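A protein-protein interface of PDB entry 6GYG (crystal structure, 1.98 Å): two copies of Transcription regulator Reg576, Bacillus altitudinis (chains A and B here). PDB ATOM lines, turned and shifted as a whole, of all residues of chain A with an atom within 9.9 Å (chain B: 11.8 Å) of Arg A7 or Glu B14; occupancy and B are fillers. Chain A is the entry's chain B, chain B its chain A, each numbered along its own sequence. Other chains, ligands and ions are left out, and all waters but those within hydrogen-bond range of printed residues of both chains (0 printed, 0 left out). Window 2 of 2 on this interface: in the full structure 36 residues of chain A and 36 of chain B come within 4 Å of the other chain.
Phe A6 touches three residues of chain B.
Of the printed residues of chain B, Arg A7 touches Glu B14 (3.9 Å).
Arg A63 touches none of the printed residues of chain B.
Lys A64 touches none of the printed residues of chain B.
Of the printed residues of chain A, Asn B9 touches Asn A9 and Ile A10.
Printed residues of chain A within 4 Å of Leu B12: Phe A6 (3.6 Å), Lys A8 (3.1 Å), Ile A10 (3.96 Å) and Tyr A32 (3.9 Å).
Thr B13 touches just these residues of chain A: Phe A6 and Tyr A32.
Of chain A, only Arg A7 (3.9 Å), Lys A8 (3.9 Å) and Glu A66 (3.7 Å) come within 4 Å of Glu B14.
The nearest residue of chain B that does not touch Arg A7 is Leu B12 (4.8 Å).
The nearest residue of chain A that does not touch Glu B14 is Phe A6 (6.3 Å).
Asn B9 touches its own counterpart, Asn A9.
Asn A9 touches Ile B10, and with the chains exchanged Ile A10 touches Asn B9.
Ile A10 touches its own counterpart, Ile B10.
Positions printed for both chains: 9 and 10.
The backbone carbonyl oxygen of Lys A8 is in hydrogen-bond range of the backbone NH of Leu B12.
The side-chain carboxylate of Glu B14 lies within salt-bridge range of the guanidinium group of Arg A7, at 3.9 Å.
The side-chain amino group (NZ) of Lys B19 is in salt-bridge range of the side-chain carboxylate (OE2) of Glu A36, 2.9 Å away.
N of Ile B10 lies within hydrogen-bond range of O of Ile A10, 2.8 Å away.
OE2 of Glu A66 lies within hydrogen-bond range of ND2 of Asn B18 (2.9 Å).
The side-chain amide nitrogen (ND2) of Asn A9 sits close to the side-chain amide nitrogen (ND2) of Asn B9 (3.1 Å).
Of the 16 printed residues of chain B, 15 touch a printed residue of chain A.
Printed residues of chain B that touch a printed residue of chain A: Asn B9, Ile B10, Lys B11, Leu B12, Thr B13, Glu B14, Ile B16, Phe B17, Asn B18, Lys B19, Leu B20, Lys B21, Ala B22, Leu B23 and Gln B31.
Hydrophobic or aromatic side chains of chain B that line the printed part of chain A: Ile B10, Leu B12, Ile B16, Phe B17, Leu B20 and Leu B23.
Of the 14 printed residues of chain A, 11 touch a printed residue of chain B.
Hydrophobic or aromatic side chains of chain A that line the printed part of chain B: Phe A6, Ile A10, Tyr A32, Leu A39, Leu A59 and Leu A62.
Along chain A the printed residues that touch a printed residue of chain B span positions 6 to 66.
Among the printed residues, 31 pairs touch across the chains.
The backbone NH (N) of Ile B16 lies close to the side-chain hydroxyl (OG1) of Thr B13 (3.5 Å).
The backbone carbonyl oxygen (O) of Glu B14 lies close to the side-chain amide oxygen (OD1) of Asn B18 (3.3 Å).
Among the printed residues, merely in contact across the chains: Phe A6 with Lys B11, Phe A6 with Leu B12, Phe A6 with Thr B13, Lys A8 with Lys B11, Lys A8 with Glu B14, Lys A8 with Phe B17, Asn A9 with Ile B10, Asn A9 with Lys B11, Ile A10 with Asn B9, Ile A10 with Leu B12, Ile A10 with Phe B17, Ile A10 with Leu B20, Ile A10 with Gln B31, Tyr A32 with Lys B11, Tyr A32 with Leu B12, Tyr A32 with Thr B13, Tyr A32 with Ile B16, Glu A36 with Ile B16, Leu A39 with Leu B23, Leu A59 with Asn B18, Leu A59 with Lys B19, Leu A62 with Asn B18, Leu A62 with Lys B21, Leu A62 with Ala B22 and Glu A66 with Glu B14.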
ATOM      1  N   PHE A   6       4.448  16.715  14.069  1.00  0.00           N
ATOM      2  CA  PHE A   6       4.636  16.292  15.505  1.00  0.00           C
ATOM      3  C   PHE A   6       5.920  15.462  15.604  1.00  0.00           C
ATOM      4  O   PHE A   6       6.051  14.377  14.998  1.00  0.00           O
ATOM      5  CB  PHE A   6       3.417  15.522  16.015  1.00  0.00           C
ATOM      6  CG  PHE A   6       2.107  16.248  15.881  1.00  0.00           C
ATOM      7  CD1 PHE A   6       1.286  16.047  14.776  1.00  0.00           C
ATOM      8  CD2 PHE A   6       1.690  17.138  16.861  1.00  0.00           C
ATOM      9  CE1 PHE A   6       0.077  16.730  14.659  1.00  0.00           C
ATOM     10  CE2 PHE A   6       0.482  17.814  16.744  1.00  0.00           C
ATOM     11  CZ  PHE A   6      -0.321  17.615  15.642  1.00  0.00           C
ATOM     12  N   ARG A   7       6.870  15.981  16.381  1.00  0.00           N
ATOM     13  CA  ARG A   7       8.213  15.416  16.483  1.00  0.00           C
ATOM     14  C   ARG A   7       8.127  14.026  17.112  1.00  0.00           C
ATOM     15  O   ARG A   7       8.850  13.088  16.737  1.00  0.00           O
ATOM     16  CB  ARG A   7       9.113  16.314  17.338  1.00  0.00           C
ATOM     17  CG  ARG A   7      10.597  16.033  17.159  1.00  0.00           C
ATOM     18  CD  ARG A   7      11.455  17.151  17.727  1.00  0.00           C
ATOM     19  NE  ARG A   7      11.664  17.008  19.164  1.00  0.00           N
ATOM     20  CZ  ARG A   7      12.547  17.711  19.870  1.00  0.00           C
ATOM     21  NH1 ARG A   7      12.814  17.356  21.118  1.00  0.00           N
ATOM     22  NH2 ARG A   7      13.157  18.756  19.329  1.00  0.00           N
ATOM     23  N   LYS A   8       7.233  13.919  18.089  1.00  0.00           N
ATOM     24  CA  LYS A   8       7.149  12.751  18.931  1.00  0.00           C
ATOM     25  C   LYS A   8       6.140  11.791  18.321  1.00  0.00           C
ATOM     26  O   LYS A   8       5.105  12.205  17.761  1.00  0.00           O
ATOM     27  CB  LYS A   8       6.819  13.193  20.352  1.00  0.00           C
ATOM     28  CG  LYS A   8       7.746  14.279  20.881  1.00  0.00           C
ATOM     29  CD  LYS A   8       9.072  13.719  21.333  1.00  0.00           C
ATOM     30  CE  LYS A   8       9.907  14.744  22.076  1.00  0.00           C
ATOM     31  NZ  LYS A   8      11.339  14.420  21.954  1.00  0.00           N
ATOM     32  N   ASN A   9       6.449  10.501  18.419  1.00  0.00           N
ATOM     33  CA  ASN A   9       5.486   9.528  18.019  1.00  0.00           C
ATOM     34  C   ASN A   9       5.762   8.191  18.726  1.00  0.00           C
ATOM     35  O   ASN A   9       6.775   7.998  19.370  1.00  0.00           O
ATOM     36  CB  ASN A   9       5.404   9.482  16.492  1.00  0.00           C
ATOM     37  CG  ASN A   9       6.606   8.819  15.867  1.00  0.00           C
ATOM     38  OD1 ASN A   9       6.918   7.667  16.197  1.00  0.00           O
ATOM     39  ND2 ASN A   9       7.288   9.549  14.991  1.00  0.00           N
ATOM     40  N   ILE A  10       4.791   7.285  18.659  1.00  0.00           N
ATOM     41  CA  ILE A  10       4.903   5.992  19.258  1.00  0.00           C
ATOM     42  C   ILE A  10       4.371   4.967  18.250  1.00  0.00           C
ATOM     43  O   ILE A  10       3.660   5.308  17.321  1.00  0.00           O
ATOM     44  CB  ILE A  10       4.163   5.956  20.624  1.00  0.00           C
ATOM     45  CG1 ILE A  10       2.650   6.074  20.477  1.00  0.00           C
ATOM     46  CG2 ILE A  10       4.686   7.017  21.605  1.00  0.00           C
ATOM     47  CD1 ILE A  10       1.893   5.770  21.780  1.00  0.00           C
ATOM     48  N   TYR A  32      -4.270  11.886  19.476  1.00  0.00           N
ATOM     49  CA  TYR A  32      -3.386  12.347  20.541  1.00  0.00           C
ATOM     50  C   TYR A  32      -4.251  12.863  21.694  1.00  0.00           C
ATOM     51  O   TYR A  32      -3.861  12.730  22.827  1.00  0.00           O
ATOM     52  CB  TYR A  32      -2.341  13.376  20.081  1.00  0.00           C
ATOM     53  CG  TYR A  32      -2.881  14.720  19.662  1.00  0.00           C
ATOM     54  CD1 TYR A  32      -3.096  15.706  20.604  1.00  0.00           C
ATOM     55  CD2 TYR A  32      -3.176  15.004  18.339  1.00  0.00           C
ATOM     56  CE1 TYR A  32      -3.614  16.935  20.264  1.00  0.00           C
ATOM     57  CE2 TYR A  32      -3.652  16.254  17.968  1.00  0.00           C
ATOM     58  CZ  TYR A  32      -3.864  17.227  18.939  1.00  0.00           C
ATOM     59  OH  TYR A  32      -4.306  18.485  18.647  1.00  0.00           O
ATOM     60  N   GLU A  36      -4.285  11.438  25.640  1.00  0.00           N
ATOM     61  CA  GLU A  36      -4.156  12.273  26.764  1.00  0.00           C
ATOM     62  C   GLU A  36      -5.283  12.003  27.745  1.00  0.00           C
ATOM     63  O   GLU A  36      -5.058  11.917  28.927  1.00  0.00           O
ATOM     64  CB  GLU A  36      -4.208  13.741  26.338  1.00  0.00           C
ATOM     65  CG  GLU A  36      -3.778  14.669  27.469  1.00  0.00           C
ATOM     66  CD  GLU A  36      -3.597  16.139  27.099  1.00  0.00           C
ATOM     67  OE1 GLU A  36      -4.150  16.576  26.045  1.00  0.00           O
ATOM     68  OE2 GLU A  36      -2.879  16.851  27.863  1.00  0.00           O
ATOM     69  N   LEU A  39      -4.706   8.754  29.529  1.00  0.00           N
ATOM     70  CA  LEU A  39      -3.615   8.952  30.485  1.00  0.00           C
ATOM     71  C   LEU A  39      -4.115   9.647  31.762  1.00  0.00           C
ATOM     72  O   LEU A  39      -3.862   9.170  32.854  1.00  0.00           O
ATOM     73  CB  LEU A  39      -2.478   9.753  29.874  1.00  0.00           C
ATOM     74  CG  LEU A  39      -1.568   8.938  28.954  1.00  0.00           C
ATOM     75  CD1 LEU A  39      -0.778   9.826  27.995  1.00  0.00           C
ATOM     76  CD2 LEU A  39      -0.614   8.132  29.798  1.00  0.00           C
ATOM     77  N   LEU A  59       7.664  14.080  35.673  1.00  0.00           N
ATOM     78  CA  LEU A  59       7.133  15.053  34.749  1.00  0.00           C
ATOM     79  C   LEU A  59       7.915  16.358  34.918  1.00  0.00           C
ATOM     80  O   LEU A  59       8.337  16.961  33.934  1.00  0.00           O
ATOM     81  CB  LEU A  59       5.647  15.212  35.063  1.00  0.00           C
ATOM     82  CG  LEU A  59       4.693  15.636  33.964  1.00  0.00           C
ATOM     83  CD1 LEU A  59       4.921  14.869  32.662  1.00  0.00           C
ATOM     84  CD2 LEU A  59       3.245  15.508  34.463  1.00  0.00           C
ATOM     85  N   LEU A  62      11.385  15.564  33.269  1.00  0.00           N
ATOM     86  CA  LEU A  62      11.347  15.631  31.796  1.00  0.00           C
ATOM     87  C   LEU A  62      11.297  17.097  31.336  1.00  0.00           C
ATOM     88  O   LEU A  62      11.885  17.420  30.326  1.00  0.00           O
ATOM     89  CB  LEU A  62      10.174  14.808  31.264  1.00  0.00           C
ATOM     90  CG  LEU A  62      10.287  13.302  31.507  1.00  0.00           C
ATOM     91  CD1 LEU A  62       8.969  12.592  31.211  1.00  0.00           C
ATOM     92  CD2 LEU A  62      11.427  12.710  30.687  1.00  0.00           C
ATOM     93  N   ARG A  63      10.678  17.989  32.122  1.00  0.00           N
ATOM     94  CA  ARG A  63      10.692  19.443  31.854  1.00  0.00           C
ATOM     95  C   ARG A  63      12.119  20.001  31.974  1.00  0.00           C
ATOM     96  O   ARG A  63      12.643  20.556  31.030  1.00  0.00           O
ATOM     97  CB  ARG A  63       9.709  20.173  32.773  1.00  0.00           C
ATOM     98  CG  ARG A  63       8.347  20.418  32.133  1.00  0.00           C
ATOM     99  CD  ARG A  63       7.150  19.854  32.880  1.00  0.00           C
ATOM    100  NE  ARG A  63       5.921  20.383  32.305  1.00  0.00           N
ATOM    101  CZ  ARG A  63       4.685  20.059  32.688  1.00  0.00           C
ATOM    102  NH1 ARG A  63       4.479  19.116  33.586  1.00  0.00           N
ATOM    103  NH2 ARG A  63       3.646  20.707  32.192  1.00  0.00           N
ATOM    104  N   LYS A  64      12.752  19.838  33.135  1.00  0.00           N
ATOM    105  CA  LYS A  64      14.162  20.243  33.324  1.00  0.00           C
ATOM    106  C   LYS A  64      15.012  19.807  32.122  1.00  0.00           C
ATOM    107  O   LYS A  64      15.681  20.621  31.501  1.00  0.00           O
ATOM    108  CB  LYS A  64      14.731  19.608  34.598  1.00  0.00           C
ATOM    109  CG  LYS A  64      15.315  20.590  35.598  1.00  0.00           C
ATOM    110  CD  LYS A  64      15.201  20.095  37.020  1.00  0.00           C
ATOM    111  CE  LYS A  64      16.130  18.930  37.299  1.00  0.00           C
ATOM    112  NZ  LYS A  64      16.388  18.795  38.752  1.00  0.00           N
ATOM    113  N   GLU A  65      14.976  18.506  31.809  1.00  0.00           N
ATOM    114  CA  GLU A  65      15.817  17.893  30.792  1.00  0.00           C
ATOM    115  C   GLU A  65      15.222  18.195  29.412  1.00  0.00           C
ATOM    116  O   GLU A  65      14.862  17.275  28.671  1.00  0.00           O
ATOM    117  CB  GLU A  65      15.938  16.389  31.060  1.00  0.00           C
ATOM    118  CG  GLU A  65      16.916  15.671  30.140  1.00  0.00           C
ATOM    119  CD  GLU A  65      17.531  14.388  30.687  1.00  0.00           C
ATOM    120  OE1 GLU A  65      16.947  13.786  31.621  1.00  0.00           O
ATOM    121  OE2 GLU A  65      18.604  13.990  30.174  1.00  0.00           O
ATOM    122  N   GLU A  66      15.114  19.491  29.081  1.00  0.00           N
ATOM    123  CA  GLU A  66      14.646  19.947  27.763  1.00  0.00           C
ATOM    124  C   GLU A  66      15.497  21.140  27.319  1.00  0.00           C
ATOM    125  O   GLU A  66      15.437  22.204  27.922  1.00  0.00           O
ATOM    126  CB  GLU A  66      13.168  20.339  27.796  1.00  0.00           C
ATOM    127  CG  GLU A  66      12.259  19.159  28.055  1.00  0.00           C
ATOM    128  CD  GLU A  66      10.786  19.439  27.804  1.00  0.00           C
ATOM    129  OE1 GLU A  66      10.390  20.623  27.896  1.00  0.00           O
ATOM    130  OE2 GLU A  66      10.051  18.481  27.491  1.00  0.00           O
ATOM    131  N   ASN B   9       2.722   5.298  12.631  1.00  0.00           N
ATOM    132  CA  ASN B   9       3.064   5.635  13.977  1.00  0.00           C
ATOM    133  C   ASN B   9       1.886   6.500  14.464  1.00  0.00           C
ATOM    134  O   ASN B   9       1.021   6.905  13.660  1.00  0.00           O
ATOM    135  CB  ASN B   9       4.503   6.152  14.091  1.00  0.00           C
ATOM    136  CG  ASN B   9       4.736   7.416  13.299  1.00  0.00           C
ATOM    137  OD1 ASN B   9       3.773   8.147  13.012  1.00  0.00           O
ATOM    138  ND2 ASN B   9       5.981   7.642  12.888  1.00  0.00           N
ATOM    139  N   ILE B  10       1.802   6.711  15.777  1.00  0.00           N
ATOM    140  CA  ILE B  10       0.831   7.626  16.368  1.00  0.00           C
ATOM    141  C   ILE B  10       1.621   8.853  16.831  1.00  0.00           C
ATOM    142  O   ILE B  10       2.579   8.753  17.603  1.00  0.00           O
ATOM    143  CB  ILE B  10       0.085   6.908  17.512  1.00  0.00           C
ATOM    144  CG1 ILE B  10      -0.830   5.816  16.967  1.00  0.00           C
ATOM    145  CG2 ILE B  10      -0.699   7.859  18.398  1.00  0.00           C
ATOM    146  CD1 ILE B  10      -0.198   4.456  16.989  1.00  0.00           C
ATOM    147  N   LYS B  11       1.188  10.018  16.380  1.00  0.00           N
ATOM    148  CA  LYS B  11       1.880  11.262  16.618  1.00  0.00           C
ATOM    149  C   LYS B  11       1.285  11.865  17.886  1.00  0.00           C
ATOM    150  O   LYS B  11       0.134  11.701  18.141  1.00  0.00           O
ATOM    151  CB  LYS B  11       1.772  12.111  15.346  1.00  0.00           C
ATOM    152  CG  LYS B  11       2.739  11.642  14.249  1.00  0.00           C
ATOM    153  CD  LYS B  11       2.232  11.826  12.844  1.00  0.00           C
ATOM    154  CE  LYS B  11       3.178  11.266  11.805  1.00  0.00           C
ATOM    155  NZ  LYS B  11       4.436  12.052  11.746  1.00  0.00           N
ATOM    156  N   LEU B  12       2.144  12.409  18.726  1.00  0.00           N
ATOM    157  CA  LEU B  12       1.768  12.982  19.981  1.00  0.00           C
ATOM    158  C   LEU B  12       2.431  14.358  20.062  1.00  0.00           C
ATOM    159  O   LEU B  12       3.437  14.562  19.448  1.00  0.00           O
ATOM    160  CB  LEU B  12       2.281  12.113  21.121  1.00  0.00           C
ATOM    161  CG  LEU B  12       1.753  10.685  21.228  1.00  0.00           C
ATOM    162  CD1 LEU B  12       2.310  10.057  22.495  1.00  0.00           C
ATOM    163  CD2 LEU B  12       0.242  10.664  21.282  1.00  0.00           C
ATOM    164  N   THR B  13       1.858  15.241  20.868  1.00  0.00           N
ATOM    165  CA  THR B  13       2.470  16.464  21.211  1.00  0.00           C
ATOM    166  C   THR B  13       3.456  16.131  22.305  1.00  0.00           C
ATOM    167  O   THR B  13       3.353  15.093  22.960  1.00  0.00           O
ATOM    168  CB  THR B  13       1.443  17.524  21.646  1.00  0.00           C
ATOM    169  OG1 THR B  13       0.940  17.148  22.919  1.00  0.00           O
ATOM    170  CG2 THR B  13       0.290  17.726  20.671  1.00  0.00           C
ATOM    171  N   GLU B  14       4.401  17.037  22.502  1.00  0.00           N
ATOM    172  CA  GLU B  14       5.456  16.849  23.473  1.00  0.00           C
ATOM    173  C   GLU B  14       4.919  16.735  24.898  1.00  0.00           C
ATOM    174  O   GLU B  14       5.353  15.808  25.600  1.00  0.00           O
ATOM    175  CB  GLU B  14       6.485  17.975  23.385  1.00  0.00           C
ATOM    176  CG  GLU B  14       7.814  17.561  23.977  1.00  0.00           C
ATOM    177  CD  GLU B  14       8.854  18.667  23.955  1.00  0.00           C
ATOM    178  OE1 GLU B  14       8.488  19.845  24.282  1.00  0.00           O
ATOM    179  OE2 GLU B  14      10.012  18.354  23.600  1.00  0.00           O
ATOM    180  N   PRO B  15       4.006  17.629  25.388  1.00  0.00           N
ATOM    181  CA  PRO B  15       3.418  17.453  26.710  1.00  0.00           C
ATOM    182  C   PRO B  15       2.743  16.068  26.837  1.00  0.00           C
ATOM    183  O   PRO B  15       2.836  15.480  27.842  1.00  0.00           O
ATOM    184  CB  PRO B  15       2.355  18.549  26.888  1.00  0.00           C
ATOM    185  CG  PRO B  15       2.391  19.368  25.629  1.00  0.00           C
ATOM    186  CD  PRO B  15       3.420  18.781  24.679  1.00  0.00           C
ATOM    187  N   ILE B  16       2.114  15.532  25.783  1.00  0.00           N
ATOM    188  CA  ILE B  16       1.409  14.245  25.934  1.00  0.00           C
ATOM    189  C   ILE B  16       2.445  13.121  25.967  1.00  0.00           C
ATOM    190  O   ILE B  16       2.316  12.162  26.758  1.00  0.00           O
ATOM    191  CB  ILE B  16       0.331  14.020  24.863  1.00  0.00           C
ATOM    192  CG1 ILE B  16      -0.716  15.132  24.906  1.00  0.00           C
ATOM    193  CG2 ILE B  16      -0.330  12.666  25.033  1.00  0.00           C
ATOM    194  CD1 ILE B  16      -1.644  15.120  23.748  1.00  0.00           C
ATOM    195  N   PHE B  17       3.463  13.228  25.106  1.00  0.00           N
ATOM    196  CA  PHE B  17       4.556  12.244  25.124  1.00  0.00           C
ATOM    197  C   PHE B  17       5.229  12.227  26.490  1.00  0.00           C
ATOM    198  O   PHE B  17       5.519  11.124  27.050  1.00  0.00           O
ATOM    199  CB  PHE B  17       5.585  12.542  24.028  1.00  0.00           C
ATOM    200  CG  PHE B  17       6.641  11.475  23.870  1.00  0.00           C
ATOM    201  CD1 PHE B  17       6.319  10.219  23.388  1.00  0.00           C
ATOM    202  CD2 PHE B  17       7.946  11.699  24.270  1.00  0.00           C
ATOM    203  CE1 PHE B  17       7.294   9.237  23.240  1.00  0.00           C
ATOM    204  CE2 PHE B  17       8.917  10.710  24.137  1.00  0.00           C
ATOM    205  CZ  PHE B  17       8.592   9.471  23.632  1.00  0.00           C
ATOM    206  N   ASN B  18       5.514  13.430  27.027  1.00  0.00           N
ATOM    207  CA  ASN B  18       6.111  13.536  28.376  1.00  0.00           C
ATOM    208  C   ASN B  18       5.234  12.789  29.417  1.00  0.00           C
ATOM    209  O   ASN B  18       5.746  12.068  30.286  1.00  0.00           O
ATOM    210  CB  ASN B  18       6.352  14.986  28.809  1.00  0.00           C
ATOM    211  CG  ASN B  18       7.484  15.649  28.046  1.00  0.00           C
ATOM    212  OD1 ASN B  18       8.142  15.018  27.232  1.00  0.00           O
ATOM    213  ND2 ASN B  18       7.698  16.938  28.258  1.00  0.00           N
ATOM    214  N   LYS B  19       3.916  12.948  29.348  1.00  0.00           N
ATOM    215  CA  LYS B  19       3.044  12.325  30.399  1.00  0.00           C
ATOM    216  C   LYS B  19       3.060  10.785  30.270  1.00  0.00           C
ATOM    217  O   LYS B  19       3.024  10.082  31.282  1.00  0.00           O
ATOM    218  CB  LYS B  19       1.603  12.805  30.293  1.00  0.00           C
ATOM    219  CG  LYS B  19       1.306  14.231  30.702  1.00  0.00           C
ATOM    220  CD  LYS B  19      -0.206  14.421  30.881  1.00  0.00           C
ATOM    221  CE  LYS B  19      -0.642  15.870  30.831  1.00  0.00           C
ATOM    222  NZ  LYS B  19      -2.090  16.013  30.540  1.00  0.00           N
ATOM    223  N   LEU B  20       3.185  10.281  29.033  1.00  0.00           N
ATOM    224  CA  LEU B  20       3.316   8.829  28.743  1.00  0.00           C
ATOM    225  C   LEU B  20       4.656   8.282  29.244  1.00  0.00           C
ATOM    226  O   LEU B  20       4.714   7.168  29.832  1.00  0.00           O
ATOM    227  CB  LEU B  20       3.203   8.565  27.244  1.00  0.00           C
ATOM    228  CG  LEU B  20       3.507   7.123  26.820  1.00  0.00           C
ATOM    229  CD1 LEU B  20       2.482   6.194  27.420  1.00  0.00           C
ATOM    230  CD2 LEU B  20       3.521   6.977  25.304  1.00  0.00           C
ATOM    231  N   LYS B  21       5.729   9.039  28.997  1.00  0.00           N
ATOM    232  CA  LYS B  21       7.068   8.677  29.485  1.00  0.00           C
ATOM    233  C   LYS B  21       7.094   8.713  31.016  1.00  0.00           C
ATOM    234  O   LYS B  21       7.645   7.872  31.638  1.00  0.00           O
ATOM    235  CB  LYS B  21       8.110   9.633  28.914  1.00  0.00           C
ATOM    236  CG  LYS B  21       9.395   8.944  28.513  1.00  0.00           C
ATOM    237  CD  LYS B  21      10.431   9.814  27.805  1.00  0.00           C
ATOM    238  CE  LYS B  21      11.841   9.429  28.231  1.00  0.00           C
ATOM    239  NZ  LYS B  21      12.869  10.147  27.443  1.00  0.00           N
ATOM    240  N   ALA B  22       6.494   9.733  31.622  1.00  0.00           N
ATOM    241  CA  ALA B  22       6.458   9.800  33.082  1.00  0.00           C
ATOM    242  C   ALA B  22       5.692   8.599  33.628  1.00  0.00           C
ATOM    243  O   ALA B  22       6.117   8.004  34.584  1.00  0.00           O
ATOM    244  CB  ALA B  22       5.866  11.088  33.580  1.00  0.00           C
ATOM    245  N   LEU B  23       4.581   8.216  33.006  1.00  0.00           N
ATOM    246  CA  LEU B  23       3.778   7.118  33.579  1.00  0.00           C
ATOM    247  C   LEU B  23       4.504   5.770  33.334  1.00  0.00           C
ATOM    248  O   LEU B  23       4.387   4.816  34.105  1.00  0.00           O
ATOM    249  CB  LEU B  23       2.387   7.154  32.953  1.00  0.00           C
ATOM    250  CG  LEU B  23       1.448   6.050  33.420  1.00  0.00           C
ATOM    251  CD1 LEU B  23       1.189   6.136  34.914  1.00  0.00           C
ATOM    252  CD2 LEU B  23       0.140   6.114  32.658  1.00  0.00           C
ATOM    253  N   GLN B  31       5.894   0.250  26.543  1.00  0.00           N
ATOM    254  CA  GLN B  31       5.148   1.421  26.150  1.00  0.00           C
ATOM    255  C   GLN B  31       3.767   1.049  25.591  1.00  0.00           C
ATOM    256  O   GLN B  31       2.742   1.590  26.052  1.00  0.00           O
ATOM    257  CB  GLN B  31       5.954   2.168  25.100  1.00  0.00           C
ATOM    258  CG  GLN B  31       5.442   3.556  24.780  1.00  0.00           C
ATOM    259  CD  GLN B  31       6.310   4.124  23.687  1.00  0.00           C
ATOM    260  OE1 GLN B  31       6.246   3.684  22.541  1.00  0.00           O
ATOM    261  NE2 GLN B  31       7.148   5.084  24.038  1.00  0.00           N
